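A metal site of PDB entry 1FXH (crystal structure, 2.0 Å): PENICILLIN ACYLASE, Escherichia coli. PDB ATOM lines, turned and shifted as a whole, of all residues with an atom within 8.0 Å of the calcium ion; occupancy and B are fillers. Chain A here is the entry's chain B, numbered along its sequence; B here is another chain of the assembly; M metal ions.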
ATOM      1  N   GLY A  72     -18.365  18.631 -15.145  1.00  0.00           N
ATOM      2  CA  GLY A  72     -17.008  18.133 -15.163  1.00  0.00           C
ATOM      3  C   GLY A  72     -16.561  17.943 -13.716  1.00  0.00           C
ATOM      4  O   GLY A  72     -17.280  18.351 -12.795  1.00  0.00           O
ATOM      5  N   ASP A  73     -15.401  17.320 -13.502  1.00  0.00           N
ATOM      6  CA  ASP A  73     -14.878  17.170 -12.147  1.00  0.00           C
ATOM      7  C   ASP A  73     -13.881  18.282 -11.848  1.00  0.00           C
ATOM      8  O   ASP A  73     -12.696  18.146 -12.142  1.00  0.00           O
ATOM      9  CB  ASP A  73     -14.182  15.813 -11.984  1.00  0.00           C
ATOM     10  CG  ASP A  73     -13.750  15.559 -10.543  1.00  0.00           C
ATOM     11  OD1 ASP A  73     -13.663  16.531  -9.770  1.00  0.00           O
ATOM     12  OD2 ASP A  73     -13.495  14.387 -10.179  1.00  0.00           O
ATOM     13  N   ASP A  74     -14.366  19.375 -11.278  1.00  0.00           N
ATOM     14  CA  ASP A  74     -13.499  20.505 -10.949  1.00  0.00           C
ATOM     15  C   ASP A  74     -13.371  20.681  -9.446  1.00  0.00           C
ATOM     16  O   ASP A  74     -12.985  21.749  -8.964  1.00  0.00           O
ATOM     17  CB  ASP A  74     -14.033  21.796 -11.607  1.00  0.00           C
ATOM     18  CG  ASP A  74     -15.455  22.126 -11.169  1.00  0.00           C
ATOM     19  OD1 ASP A  74     -16.039  21.372 -10.376  1.00  0.00           O
ATOM     20  OD2 ASP A  74     -15.991  23.162 -11.614  1.00  0.00           O
ATOM     21  N   VAL A  75     -13.694  19.625  -8.703  1.00  0.00           N
ATOM     22  CA  VAL A  75     -13.629  19.674  -7.243  1.00  0.00           C
ATOM     23  C   VAL A  75     -13.017  18.403  -6.664  1.00  0.00           C
ATOM     24  O   VAL A  75     -13.515  17.305  -6.883  1.00  0.00           O
ATOM     25  CB  VAL A  75     -15.023  19.856  -6.626  1.00  0.00           C
ATOM     26  CG1 VAL A  75     -14.904  19.943  -5.108  1.00  0.00           C
ATOM     27  CG2 VAL A  75     -15.684  21.115  -7.190  1.00  0.00           C
ATOM     28  N   ASP A  76     -11.925  18.559  -5.918  1.00  0.00           N
ATOM     29  CA  ASP A  76     -11.293  17.439  -5.242  1.00  0.00           C
ATOM     30  C   ASP A  76     -11.200  17.716  -3.739  1.00  0.00           C
ATOM     31  O   ASP A  76     -11.137  18.877  -3.313  1.00  0.00           O
ATOM     32  CB  ASP A  76      -9.874  17.207  -5.783  1.00  0.00           C
ATOM     33  CG  ASP A  76      -9.856  16.717  -7.221  1.00  0.00           C
ATOM     34  OD1 ASP A  76     -10.876  16.198  -7.716  1.00  0.00           O
ATOM     35  OD2 ASP A  76      -8.787  16.845  -7.864  1.00  0.00           O
ATOM     36  N   ILE A  77     -11.179  16.646  -2.960  1.00  0.00           N
ATOM     37  CA  ILE A  77     -11.096  16.766  -1.506  1.00  0.00           C
ATOM     38  C   ILE A  77      -9.715  16.391  -1.006  1.00  0.00           C
ATOM     39  O   ILE A  77      -9.209  15.308  -1.302  1.00  0.00           O
ATOM     40  CB  ILE A  77     -12.135  15.866  -0.823  1.00  0.00           C
ATOM     41  CG1 ILE A  77     -13.544  16.403  -1.092  1.00  0.00           C
ATOM     42  CG2 ILE A  77     -11.850  15.783   0.671  1.00  0.00           C
ATOM     43  CD1 ILE A  77     -14.592  15.731  -0.276  1.00  0.00           C
ATOM     44  N   SER A 140     -11.370  21.490  -2.484  1.00  0.00           N
ATOM     45  CA  SER A 140     -10.593  22.259  -3.440  1.00  0.00           C
ATOM     46  C   SER A 140     -11.323  22.441  -4.765  1.00  0.00           C
ATOM     47  O   SER A 140     -11.551  21.478  -5.492  1.00  0.00           O
ATOM     48  CB  SER A 140      -9.236  21.578  -3.683  1.00  0.00           C
ATOM     49  OG  SER A 140      -8.446  22.327  -4.589  1.00  0.00           O
ATOM     50  N   PRO A 197      -8.344  20.986 -12.828  1.00  0.00           N
ATOM     51  CA  PRO A 197      -7.017  20.773 -12.266  1.00  0.00           C
ATOM     52  C   PRO A 197      -6.103  19.897 -13.114  1.00  0.00           C
ATOM     53  O   PRO A 197      -6.553  18.953 -13.764  1.00  0.00           O
ATOM     54  CB  PRO A 197      -7.330  20.151 -10.909  1.00  0.00           C
ATOM     55  CG  PRO A 197      -8.506  19.298 -11.212  1.00  0.00           C
ATOM     56  CD  PRO A 197      -9.364  20.216 -12.093  1.00  0.00           C
ATOM     57  N   ARG A 199      -3.814  17.356 -12.405  1.00  0.00           N
ATOM     58  CA  ARG A 199      -3.548  16.516 -11.236  1.00  0.00           C
ATOM     59  C   ARG A 199      -2.223  15.753 -11.351  1.00  0.00           C
ATOM     60  O   ARG A 199      -1.768  15.454 -12.452  1.00  0.00           O
ATOM     61  CB  ARG A 199      -4.689  15.520 -11.033  1.00  0.00           C
ATOM     62  CG  ARG A 199      -6.062  16.174 -10.916  1.00  0.00           C
ATOM     63  CD  ARG A 199      -7.109  15.142 -10.563  1.00  0.00           C
ATOM     64  NE  ARG A 199      -8.393  15.738 -10.219  1.00  0.00           N
ATOM     65  CZ  ARG A 199      -9.353  16.049 -11.097  1.00  0.00           C
ATOM     66  NH1 ARG A 199      -9.194  15.811 -12.388  1.00  0.00           N
ATOM     67  NH2 ARG A 199     -10.488  16.573 -10.659  1.00  0.00           N
ATOM     68  N   HIS A 203      -3.291  10.355  -9.542  1.00  0.00           N
ATOM     69  CA  HIS A 203      -4.364  10.941  -8.751  1.00  0.00           C
ATOM     70  C   HIS A 203      -5.711  10.498  -9.294  1.00  0.00           C
ATOM     71  O   HIS A 203      -6.104  10.865 -10.400  1.00  0.00           O
ATOM     72  CB  HIS A 203      -4.236  12.473  -8.771  1.00  0.00           C
ATOM     73  CG  HIS A 203      -5.297  13.194  -7.993  1.00  0.00           C
ATOM     74  ND1 HIS A 203      -5.167  14.522  -7.631  1.00  0.00           N
ATOM     75  CD2 HIS A 203      -6.509  12.794  -7.542  1.00  0.00           C
ATOM     76  CE1 HIS A 203      -6.260  14.906  -6.990  1.00  0.00           C
ATOM     77  NE2 HIS A 203      -7.082  13.874  -6.924  1.00  0.00           N
ATOM     78  N   ASP A 204      -6.425   9.682  -8.516  1.00  0.00           N
ATOM     79  CA  ASP A 204      -7.774   9.247  -8.873  1.00  0.00           C
ATOM     80  C   ASP A 204      -8.734  10.349  -8.430  1.00  0.00           C
ATOM     81  O   ASP A 204      -8.949  10.559  -7.233  1.00  0.00           O
ATOM     82  CB  ASP A 204      -8.110   7.949  -8.136  1.00  0.00           C
ATOM     83  CG  ASP A 204      -9.372   7.289  -8.657  1.00  0.00           C
ATOM     84  OD1 ASP A 204     -10.332   8.030  -8.991  1.00  0.00           O
ATOM     85  OD2 ASP A 204      -9.416   6.046  -8.713  1.00  0.00           O
ATOM     86  N   PRO A 205      -9.336  11.088  -9.385  1.00  0.00           N
ATOM     87  CA  PRO A 205     -10.232  12.202  -9.061  1.00  0.00           C
ATOM     88  C   PRO A 205     -11.540  11.824  -8.380  1.00  0.00           C
ATOM     89  O   PRO A 205     -12.323  12.696  -8.000  1.00  0.00           O
ATOM     90  CB  PRO A 205     -10.455  12.868 -10.424  1.00  0.00           C
ATOM     91  CG  PRO A 205     -10.436  11.699 -11.356  1.00  0.00           C
ATOM     92  CD  PRO A 205      -9.266  10.871 -10.842  1.00  0.00           C
ATOM     93  N   ARG A 206     -11.785  10.526  -8.224  1.00  0.00           N
ATOM     94  CA  ARG A 206     -13.018  10.035  -7.614  1.00  0.00           C
ATOM     95  C   ARG A 206     -12.862   9.880  -6.098  1.00  0.00           C
ATOM     96  O   ARG A 206     -13.847   9.674  -5.389  1.00  0.00           O
ATOM     97  CB  ARG A 206     -13.393   8.688  -8.223  1.00  0.00           C
ATOM     98  CG  ARG A 206     -13.633   8.717  -9.721  1.00  0.00           C
ATOM     99  CD  ARG A 206     -13.783   7.322 -10.281  1.00  0.00           C
ATOM    100  NE  ARG A 206     -12.590   6.512 -10.040  1.00  0.00           N
ATOM    101  CZ  ARG A 206     -12.486   5.235 -10.362  1.00  0.00           C
ATOM    102  NH1 ARG A 206     -13.503   4.602 -10.944  1.00  0.00           N
ATOM    103  NH2 ARG A 206     -11.351   4.578 -10.123  1.00  0.00           N
ATOM    104  N   LEU A 207     -11.629   9.970  -5.620  1.00  0.00           N
ATOM    105  CA  LEU A 207     -11.334   9.718  -4.201  1.00  0.00           C
ATOM    106  C   LEU A 207     -10.466  10.827  -3.620  1.00  0.00           C
ATOM    107  O   LEU A 207      -9.741  11.498  -4.336  1.00  0.00           O
ATOM    108  CB  LEU A 207     -10.615   8.378  -4.072  1.00  0.00           C
ATOM    109  CG  LEU A 207     -11.360   7.207  -4.726  1.00  0.00           C
ATOM    110  CD1 LEU A 207     -10.487   5.979  -4.714  1.00  0.00           C
ATOM    111  CD2 LEU A 207     -12.672   6.953  -3.994  1.00  0.00           C
ATOM    112  N   PRO A 208     -10.547  11.040  -2.291  1.00  0.00           N
ATOM    113  CA  PRO A 208      -9.755  12.096  -1.658  1.00  0.00           C
ATOM    114  C   PRO A 208      -8.253  11.866  -1.833  1.00  0.00           C
ATOM    115  O   PRO A 208      -7.832  10.757  -2.138  1.00  0.00           O
ATOM    116  CB  PRO A 208     -10.160  11.988  -0.186  1.00  0.00           C
ATOM    117  CG  PRO A 208     -11.530  11.398  -0.238  1.00  0.00           C
ATOM    118  CD  PRO A 208     -11.382  10.347  -1.307  1.00  0.00           C
ATOM    119  N   TRP A 217      -2.416  19.865  -6.665  1.00  0.00           N
ATOM    120  CA  TRP A 217      -2.504  20.026  -8.113  1.00  0.00           C
ATOM    121  C   TRP A 217      -1.250  20.736  -8.621  1.00  0.00           C
ATOM    122  O   TRP A 217      -0.652  21.530  -7.905  1.00  0.00           O
ATOM    123  CB  TRP A 217      -3.729  20.862  -8.487  1.00  0.00           C
ATOM    124  CG  TRP A 217      -5.043  20.265  -8.069  1.00  0.00           C
ATOM    125  CD1 TRP A 217      -5.325  18.945  -7.884  1.00  0.00           C
ATOM    126  CD2 TRP A 217      -6.284  20.970  -7.901  1.00  0.00           C
ATOM    127  NE1 TRP A 217      -6.662  18.777  -7.605  1.00  0.00           N
ATOM    128  CE2 TRP A 217      -7.274  19.999  -7.609  1.00  0.00           C
ATOM    129  CE3 TRP A 217      -6.642  22.320  -7.959  1.00  0.00           C
ATOM    130  CZ2 TRP A 217      -8.613  20.349  -7.389  1.00  0.00           C
ATOM    131  CZ3 TRP A 217      -7.982  22.661  -7.744  1.00  0.00           C
ATOM    132  CH2 TRP A 217      -8.947  21.675  -7.454  1.00  0.00           C
ATOM    133  N   ALA A 250     -16.416  12.526 -16.161  1.00  0.00           N
ATOM    134  CA  ALA A 250     -17.512  13.208 -15.504  1.00  0.00           C
ATOM    135  C   ALA A 250     -17.200  13.586 -14.060  1.00  0.00           C
ATOM    136  O   ALA A 250     -16.218  13.127 -13.474  1.00  0.00           O
ATOM    137  CB  ALA A 250     -18.750  12.325 -15.540  1.00  0.00           C
ATOM    138  N   SER A 251     -18.081  14.421 -13.509  1.00  0.00           N
ATOM    139  CA  SER A 251     -18.099  14.753 -12.084  1.00  0.00           C
ATOM    140  C   SER A 251     -17.895  13.490 -11.254  1.00  0.00           C
ATOM    141  O   SER A 251     -18.293  12.397 -11.670  1.00  0.00           O
ATOM    142  CB  SER A 251     -19.455  15.378 -11.747  1.00  0.00           C
ATOM    143  OG  SER A 251     -19.667  15.435 -10.354  1.00  0.00           O
ATOM    144  N   ASP A 252     -17.286  13.624 -10.085  1.00  0.00           N
ATOM    145  CA  ASP A 252     -17.031  12.449  -9.261  1.00  0.00           C
ATOM    146  C   ASP A 252     -18.255  11.984  -8.461  1.00  0.00           C
ATOM    147  O   ASP A 252     -18.189  10.977  -7.760  1.00  0.00           O
ATOM    148  CB  ASP A 252     -15.849  12.673  -8.300  1.00  0.00           C
ATOM    149  CG  ASP A 252     -16.095  13.796  -7.321  1.00  0.00           C
ATOM    150  OD1 ASP A 252     -17.195  13.852  -6.740  1.00  0.00           O
ATOM    151  OD2 ASP A 252     -15.179  14.620  -7.126  1.00  0.00           O
ATOM    152  N   LEU A 253     -19.370  12.706  -8.577  1.00  0.00           N
ATOM    153  CA  LEU A 253     -20.591  12.344  -7.851  1.00  0.00           C
ATOM    154  C   LEU A 253     -21.003  10.907  -8.141  1.00  0.00           C
ATOM    155  O   LEU A 253     -21.197  10.532  -9.291  1.00  0.00           O
ATOM    156  CB  LEU A 253     -21.740  13.274  -8.247  1.00  0.00           C
ATOM    157  CG  LEU A 253     -21.691  14.732  -7.782  1.00  0.00           C
ATOM    158  CD1 LEU A 253     -22.883  15.472  -8.359  1.00  0.00           C
ATOM    159  CD2 LEU A 253     -21.703  14.787  -6.270  1.00  0.00           C
ATOM    160  N   SER B 149     -19.752  20.421  -6.849  1.00  0.00           N
ATOM    161  CA  SER B 149     -20.215  19.063  -6.545  1.00  0.00           C
ATOM    162  C   SER B 149     -19.087  18.056  -6.428  1.00  0.00           C
ATOM    163  O   SER B 149     -18.264  17.910  -7.327  1.00  0.00           O
ATOM    164  CB  SER B 149     -21.183  18.590  -7.628  1.00  0.00           C
ATOM    165  OG  SER B 149     -22.258  19.497  -7.789  1.00  0.00           O
ATOM    166  N   THR B 150     -19.061  17.356  -5.301  1.00  0.00           N
ATOM    167  CA  THR B 150     -18.125  16.251  -5.100  1.00  0.00           C
ATOM    168  C   THR B 150     -18.699  15.299  -4.060  1.00  0.00           C
ATOM    169  O   THR B 150     -19.448  15.715  -3.183  1.00  0.00           O
ATOM    170  CB  THR B 150     -16.742  16.764  -4.609  1.00  0.00           C
ATOM    171  OG1 THR B 150     -15.829  15.667  -4.532  1.00  0.00           O
ATOM    172  CG2 THR B 150     -16.865  17.402  -3.228  1.00  0.00           C
ATOM    173  N   SER B 151     -18.375  14.015  -4.180  1.00  0.00           N
ATOM    174  CA  SER B 151     -18.776  13.044  -3.160  1.00  0.00           C
ATOM    175  C   SER B 151     -17.628  12.092  -2.885  1.00  0.00           C
ATOM    176  O   SER B 151     -17.836  10.922  -2.559  1.00  0.00           O
ATOM    177  CB  SER B 151     -20.002  12.253  -3.630  1.00  0.00           C
ATOM    178  OG  SER B 151     -19.697  11.441  -4.754  1.00  0.00           O
ATOM    179  N   GLU B 152     -16.406  12.602  -3.009  1.00  0.00           N
ATOM    180  CA  GLU B 152     -15.201  11.776  -2.864  1.00  0.00           C
ATOM    181  C   GLU B 152     -15.140  11.030  -1.533  1.00  0.00           C
ATOM    182  O   GLU B 152     -14.720   9.875  -1.485  1.00  0.00           O
ATOM    183  CB  GLU B 152     -13.958  12.636  -3.029  1.00  0.00           C
ATOM    184  CG  GLU B 152     -13.700  13.052  -4.478  1.00  0.00           C
ATOM    185  CD  GLU B 152     -12.444  13.882  -4.616  1.00  0.00           C
ATOM    186  OE1 GLU B 152     -11.680  13.988  -3.625  1.00  0.00           O
ATOM    187  OE2 GLU B 152     -12.218  14.430  -5.703  1.00  0.00           O
ATOM    188  N   ASN B 155     -17.505   8.315  -1.926  1.00  0.00           N
ATOM    189  CA  ASN B 155     -16.925   7.421  -2.918  1.00  0.00           C
ATOM    190  C   ASN B 155     -15.931   6.462  -2.268  1.00  0.00           C
ATOM    191  O   ASN B 155     -15.987   5.254  -2.498  1.00  0.00           O
ATOM    192  CB  ASN B 155     -16.191   8.236  -3.997  1.00  0.00           C
ATOM    193  CG  ASN B 155     -17.144   9.031  -4.877  1.00  0.00           C
ATOM    194  OD1 ASN B 155     -16.705   9.743  -5.792  1.00  0.00           O
ATOM    195  ND2 ASN B 155     -18.437   8.916  -4.624  1.00  0.00           N
HETATM  196 CA    CA M   1     -12.899  15.069  -7.712  1.00  0.00          CA
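N of Glu 152 of chain B lies close to OG1 of Thr 150 of chain B. The backbone NH of Ile 77 sits at hydrogen-bond distance from the side-chain carboxylate of Glu 152 of chain B, at 2.8 Å. The side-chain carboxylate (OD2) of Asp 76 is in salt-bridge range of the guanidinium group (NE) of Arg 199 (2.6 Å). The side-chain carboxylate (OD2) of Asp 76 lies within hydrogen-bond range of the indole nitrogen (NE1) of Trp 217 (2.9 Å). The backbone carbonyl oxygen of Asp 76 sits at hydrogen-bond distance from the backbone NH of Ser 140 (2.8 Å). The side-chain carboxylate (OD1) of Asp 252 sits close to the side-chain hydroxyl (OG1) of Thr 150 of chain B, at 3.2 Å. The side-chain carboxylate (OD1) of Asp 252 is in hydrogen-bond range of the backbone NH (N) of Ser 151 of chain B, at 2.8 Å. The backbone carbonyl oxygen (O) of Asp 252 sits close to the side-chain amide oxygen (OD1) of Asn 155 of chain B (2.8 Å).
Of the 25 residues printed, 6 come within 4 Å of the calcium ion.
The calcium ion is bound by OE2 of Glu 152 of chain B (2.2 Å), OD1 of Asp 76 (2.3 Å), OD2 of Asp 252 (2.4 Å), O of Pro 205 (2.5 Å), O of Val 75 (2.5 Å), OD2 of Asp 73 (2.6 Å) and OD1 of Asp 73 (2.6 Å). The calcium ion has seven donor atoms within binding distance.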
